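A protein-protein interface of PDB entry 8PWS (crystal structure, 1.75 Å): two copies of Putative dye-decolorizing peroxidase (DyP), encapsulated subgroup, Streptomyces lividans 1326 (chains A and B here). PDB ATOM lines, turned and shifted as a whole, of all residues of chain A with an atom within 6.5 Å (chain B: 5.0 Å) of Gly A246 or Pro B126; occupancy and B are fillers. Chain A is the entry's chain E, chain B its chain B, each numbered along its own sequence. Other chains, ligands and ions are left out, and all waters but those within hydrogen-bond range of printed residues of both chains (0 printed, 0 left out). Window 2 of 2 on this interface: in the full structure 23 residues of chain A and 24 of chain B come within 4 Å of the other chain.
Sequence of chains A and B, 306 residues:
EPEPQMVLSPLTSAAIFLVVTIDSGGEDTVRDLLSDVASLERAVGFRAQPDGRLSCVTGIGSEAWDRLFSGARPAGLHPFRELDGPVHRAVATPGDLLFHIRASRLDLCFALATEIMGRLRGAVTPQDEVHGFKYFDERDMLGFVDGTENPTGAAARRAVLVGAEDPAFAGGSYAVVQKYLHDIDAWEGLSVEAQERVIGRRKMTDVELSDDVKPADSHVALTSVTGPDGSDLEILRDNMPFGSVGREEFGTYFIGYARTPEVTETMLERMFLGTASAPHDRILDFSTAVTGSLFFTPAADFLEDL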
ATOM      1  N   SER A 244     -12.305 -29.741 -27.732  1.00  0.00           N
ATOM      2  CA  SER A 244     -13.441 -29.135 -27.086  1.00  0.00           C
ATOM      3  C   SER A 244     -14.218 -30.247 -26.375  1.00  0.00           C
ATOM      4  O   SER A 244     -14.644 -31.200 -27.026  1.00  0.00           O
ATOM      5  CB  SER A 244     -14.230 -28.401 -28.133  1.00  0.00           C
ATOM      6  OG  SER A 244     -15.559 -28.285 -27.684  1.00  0.00           O
ATOM      7  N   VAL A 245     -14.382 -30.146 -25.052  1.00  0.00           N
ATOM      8  CA  VAL A 245     -15.008 -31.273 -24.348  1.00  0.00           C
ATOM      9  C   VAL A 245     -16.510 -31.302 -24.605  1.00  0.00           C
ATOM     10  O   VAL A 245     -17.097 -32.358 -24.636  1.00  0.00           O
ATOM     11  CB  VAL A 245     -14.733 -31.353 -22.835  1.00  0.00           C
ATOM     12  CG1 VAL A 245     -13.266 -31.552 -22.567  1.00  0.00           C
ATOM     13  CG2 VAL A 245     -15.205 -30.148 -22.064  1.00  0.00           C
ATOM     14  N   GLY A 246     -17.127 -30.150 -24.787  1.00  0.00           N
ATOM     15  CA  GLY A 246     -18.564 -30.093 -24.990  1.00  0.00           C
ATOM     16  C   GLY A 246     -18.993 -30.698 -26.321  1.00  0.00           C
ATOM     17  O   GLY A 246     -20.036 -31.298 -26.438  1.00  0.00           O
ATOM     18  N   ARG A 247     -18.182 -30.512 -27.339  1.00  0.00           N
ATOM     19  CA  ARG A 247     -18.435 -31.079 -28.647  1.00  0.00           C
ATOM     20  C   ARG A 247     -17.811 -32.471 -28.782  1.00  0.00           C
ATOM     21  O   ARG A 247     -17.884 -33.036 -29.830  1.00  0.00           O
ATOM     22  CB  ARG A 247     -17.900 -30.133 -29.727  1.00  0.00           C
ATOM     23  CG  ARG A 247     -18.644 -28.800 -29.746  1.00  0.00           C
ATOM     24  CD  ARG A 247     -18.721 -28.126 -31.100  1.00  0.00           C
ATOM     25  NE  ARG A 247     -17.383 -28.051 -31.667  1.00  0.00           N
ATOM     26  CZ  ARG A 247     -16.393 -27.286 -31.207  1.00  0.00           C
ATOM     27  NH1 ARG A 247     -16.644 -26.339 -30.320  1.00  0.00           N
ATOM     28  NH2 ARG A 247     -15.155 -27.455 -31.649  1.00  0.00           N
ATOM     29  N   GLU A 248     -17.181 -33.036 -27.764  1.00  0.00           N
ATOM     30  CA  GLU A 248     -16.510 -34.323 -27.891  1.00  0.00           C
ATOM     31  C   GLU A 248     -15.487 -34.344 -29.037  1.00  0.00           C
ATOM     32  O   GLU A 248     -15.376 -35.326 -29.741  1.00  0.00           O
ATOM     33  CB  GLU A 248     -17.517 -35.437 -28.172  1.00  0.00           C
ATOM     34  CG  GLU A 248     -18.237 -35.919 -26.963  1.00  0.00           C
ATOM     35  CD  GLU A 248     -19.365 -36.889 -27.317  1.00  0.00           C
ATOM     36  OE1 GLU A 248     -19.088 -37.992 -27.863  1.00  0.00           O
ATOM     37  OE2 GLU A 248     -20.531 -36.530 -27.074  1.00  0.00           O
ATOM     38  N   GLU A 249     -14.715 -33.284 -29.215  1.00  0.00           N
ATOM     39  CA  GLU A 249     -13.663 -33.204 -30.210  1.00  0.00           C
ATOM     40  C   GLU A 249     -12.316 -33.339 -29.511  1.00  0.00           C
ATOM     41  O   GLU A 249     -11.955 -32.506 -28.674  1.00  0.00           O
ATOM     42  CB  GLU A 249     -13.678 -31.864 -30.933  1.00  0.00           C
ATOM     43  CG  GLU A 249     -14.539 -31.893 -32.157  1.00  0.00           C
ATOM     44  CD  GLU A 249     -14.658 -30.513 -32.776  1.00  0.00           C
ATOM     45  OE1 GLU A 249     -15.806 -30.185 -33.208  1.00  0.00           O
ATOM     46  OE2 GLU A 249     -13.592 -29.758 -32.780  1.00  0.00           O
ATOM     47  N   VAL B  19     -20.482 -24.657 -18.522  1.00  0.00           N
ATOM     48  CA  VAL B  19     -21.855 -24.503 -18.049  1.00  0.00           C
ATOM     49  C   VAL B  19     -22.729 -25.497 -18.775  1.00  0.00           C
ATOM     50  O   VAL B  19     -22.692 -25.579 -19.998  1.00  0.00           O
ATOM     51  CB  VAL B  19     -22.393 -23.093 -18.273  1.00  0.00           C
ATOM     52  CG1 VAL B  19     -23.851 -22.966 -17.791  1.00  0.00           C
ATOM     53  CG2 VAL B  19     -21.506 -22.066 -17.584  1.00  0.00           C
ATOM     54  N   VAL B  20     -23.481 -26.277 -18.013  1.00  0.00           N
ATOM     55  CA  VAL B  20     -24.325 -27.313 -18.581  1.00  0.00           C
ATOM     56  C   VAL B  20     -25.717 -27.214 -17.940  1.00  0.00           C
ATOM     57  O   VAL B  20     -25.883 -26.703 -16.829  1.00  0.00           O
ATOM     58  CB  VAL B  20     -23.730 -28.725 -18.400  1.00  0.00           C
ATOM     59  CG1 VAL B  20     -22.306 -28.793 -18.919  1.00  0.00           C
ATOM     60  CG2 VAL B  20     -23.738 -29.193 -16.946  1.00  0.00           C
ATOM     61  N   MET B 117     -16.759 -34.470 -17.889  1.00  0.00           N
ATOM     62  CA  MET B 117     -17.778 -34.618 -18.921  1.00  0.00           C
ATOM     63  C   MET B 117     -17.961 -36.073 -19.318  1.00  0.00           C
ATOM     64  O   MET B 117     -19.054 -36.440 -19.705  1.00  0.00           O
ATOM     65  CB  MET B 117     -17.450 -33.814 -20.179  1.00  0.00           C
ATOM     66  CG  MET B 117     -17.697 -32.373 -19.946  1.00  0.00           C
ATOM     67  SD  MET B 117     -19.432 -31.912 -19.663  1.00  0.00           S
ATOM     68  CE  MET B 117     -20.238 -32.734 -21.043  1.00  0.00           C
ATOM     69  N   ARG B 121     -21.729 -37.701 -19.599  1.00  0.00           N
ATOM     70  CA  ARG B 121     -22.233 -37.973 -20.944  1.00  0.00           C
ATOM     71  C   ARG B 121     -23.653 -38.544 -20.842  1.00  0.00           C
ATOM     72  O   ARG B 121     -23.929 -39.465 -20.096  1.00  0.00           O
ATOM     73  CB  ARG B 121     -21.454 -39.074 -21.692  1.00  0.00           C
ATOM     74  CG  ARG B 121     -20.154 -38.714 -22.391  1.00  0.00           C
ATOM     75  CD  ARG B 121     -20.184 -37.761 -23.572  1.00  0.00           C
ATOM     76  NE  ARG B 121     -18.863 -37.132 -23.780  1.00  0.00           N
ATOM     77  CZ  ARG B 121     -18.557 -35.834 -23.591  1.00  0.00           C
ATOM     78  NH1 ARG B 121     -17.302 -35.402 -23.723  1.00  0.00           N
ATOM     79  NH2 ARG B 121     -19.494 -34.953 -23.260  1.00  0.00           N
ATOM     80  N   VAL B 124     -26.349 -34.538 -19.292  1.00  0.00           N
ATOM     81  CA  VAL B 124     -26.304 -33.089 -19.342  1.00  0.00           C
ATOM     82  C   VAL B 124     -26.169 -32.642 -20.797  1.00  0.00           C
ATOM     83  O   VAL B 124     -25.766 -33.396 -21.664  1.00  0.00           O
ATOM     84  CB  VAL B 124     -25.170 -32.497 -18.490  1.00  0.00           C
ATOM     85  CG1 VAL B 124     -25.272 -32.932 -17.044  1.00  0.00           C
ATOM     86  CG2 VAL B 124     -23.770 -32.805 -19.044  1.00  0.00           C
ATOM     87  N   THR B 125     -26.466 -31.377 -21.037  1.00  0.00           N
ATOM     88  CA  THR B 125     -26.305 -30.747 -22.332  1.00  0.00           C
ATOM     89  C   THR B 125     -25.393 -29.562 -22.109  1.00  0.00           C
ATOM     90  O   THR B 125     -25.676 -28.740 -21.255  1.00  0.00           O
ATOM     91  CB  THR B 125     -27.657 -30.292 -22.904  1.00  0.00           C
ATOM     92  OG1 THR B 125     -28.405 -31.479 -23.102  1.00  0.00           O
ATOM     93  CG2 THR B 125     -27.543 -29.505 -24.190  1.00  0.00           C
ATOM     94  N   PRO B 126     -24.293 -29.428 -22.846  1.00  0.00           N
ATOM     95  CA  PRO B 126     -23.424 -28.262 -22.684  1.00  0.00           C
ATOM     96  C   PRO B 126     -24.149 -26.996 -23.137  1.00  0.00           C
ATOM     97  O   PRO B 126     -24.824 -27.018 -24.136  1.00  0.00           O
ATOM     98  CB  PRO B 126     -22.210 -28.546 -23.576  1.00  0.00           C
ATOM     99  CG  PRO B 126     -22.395 -29.945 -24.111  1.00  0.00           C
ATOM    100  CD  PRO B 126     -23.853 -30.334 -23.908  1.00  0.00           C
ATOM    101  N   GLN B 127     -24.017 -25.911 -22.388  1.00  0.00           N
ATOM    102  CA  GLN B 127     -24.513 -24.605 -22.807  1.00  0.00           C
ATOM    103  C   GLN B 127     -23.372 -23.656 -23.162  1.00  0.00           C
ATOM    104  O   GLN B 127     -23.540 -22.793 -23.993  1.00  0.00           O
ATOM    105  CB  GLN B 127     -25.269 -23.858 -21.710  1.00  0.00           C
ATOM    106  CG  GLN B 127     -26.501 -24.592 -21.248  1.00  0.00           C
ATOM    107  CD  GLN B 127     -27.527 -24.715 -22.353  1.00  0.00           C
ATOM    108  OE1 GLN B 127     -27.717 -23.770 -23.096  1.00  0.00           O
ATOM    109  NE2 GLN B 127     -28.126 -25.894 -22.494  1.00  0.00           N
ATOM    110  N   ASP B 128     -22.238 -23.750 -22.487  1.00  0.00           N
ATOM    111  CA  ASP B 128     -21.135 -22.851 -22.777  1.00  0.00           C
ATOM    112  C   ASP B 128     -19.850 -23.552 -22.368  1.00  0.00           C
ATOM    113  O   ASP B 128     -19.816 -24.301 -21.394  1.00  0.00           O
ATOM    114  CB  ASP B 128     -21.326 -21.525 -22.034  1.00  0.00           C
ATOM    115  CG  ASP B 128     -20.567 -20.346 -22.602  1.00  0.00           C
ATOM    116  OD1 ASP B 128     -20.127 -20.467 -23.721  1.00  0.00           O
ATOM    117  OD2 ASP B 128     -20.444 -19.321 -21.910  1.00  0.00           O
ATOM    118  N   GLU B 129     -18.794 -23.329 -23.135  1.00  0.00           N
ATOM    119  CA  GLU B 129     -17.456 -23.830 -22.853  1.00  0.00           C
ATOM    120  C   GLU B 129     -16.489 -22.742 -23.298  1.00  0.00           C
ATOM    121  O   GLU B 129     -16.482 -22.393 -24.463  1.00  0.00           O
ATOM    122  CB  GLU B 129     -17.168 -25.120 -23.613  1.00  0.00           C
ATOM    123  CG  GLU B 129     -15.782 -25.648 -23.415  1.00  0.00           C
ATOM    124  CD  GLU B 129     -15.463 -26.938 -24.156  1.00  0.00           C
ATOM    125  OE1 GLU B 129     -16.328 -27.415 -24.879  1.00  0.00           O
ATOM    126  OE2 GLU B 129     -14.308 -27.417 -24.070  1.00  0.00           O
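Among the printed residues, merely in contact across the chains: Val A245 with Met B117 (3.96 Å) and Gly A246 with Pro B126 (3.6 Å).
Gly A246 touches just these residues of chain B: Pro B126 and Glu B129. Pro B126 touches just one residue of chain A: Gly A246. Of the printed residues of chain A, Arg B121 touches Val A245 and Glu A248. Printed residues of chain B within 4 Å of Ser A244: Glu B129 (3.0 Å). Of the printed residues of chain B, Glu A248 touches Arg B121. Printed residues of chain A within 4 Å of Met B117: Val A245 (3.96 Å). Printed residues of chain B within 4 Å of Val A245: Met B117 (3.96 Å), Arg B121 (3.2 Å) and Glu B129 (2.9 Å). The nearest residue of chain B that does not touch Gly A246 is Arg B121 (4.9 Å). The nearest printed residue of chain B that does not touch Glu A248 is Glu B129 (6.4 Å).
No position is printed for both chains.
N of Ser A244 is in hydrogen-bond range of O of Glu A249, 2.9 Å away. The side-chain hydroxyl (OG) of Ser A244 sits at hydrogen-bond distance from the guanidinium group (NH1) of Arg A247 (3.5 Å).
Of the 6 printed residues of chain A, 4 touch a printed residue of chain B. Hydrophobic or aromatic side chains of chain A that line the printed part of chain B: Val A245. Along chain B the printed residues that touch a printed residue of chain A span positions 117 to 129. Among the printed residues, Asp or Glu carboxylates within 4 Å of a Lys or Arg side-chain nitrogen of the other chain: Glu A248 with Arg B121 (3.7 Å).
N of Val A245 sits at hydrogen-bond distance from OE2 of Glu B129. NH1 of Arg B121 sits at hydrogen-bond distance from O of Val A245 (3.2 Å). The guanidinium group of Arg B121 is in salt-bridge range of the side-chain carboxylate of Glu A248, 3.7 Å away. OG of Ser A244 lies within hydrogen-bond range of OE1 of Glu B129, at 3.0 Å. The side-chain carboxylate (OE1) of Glu B129 is in hydrogen-bond range of the backbone NH (N) of Gly A246.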
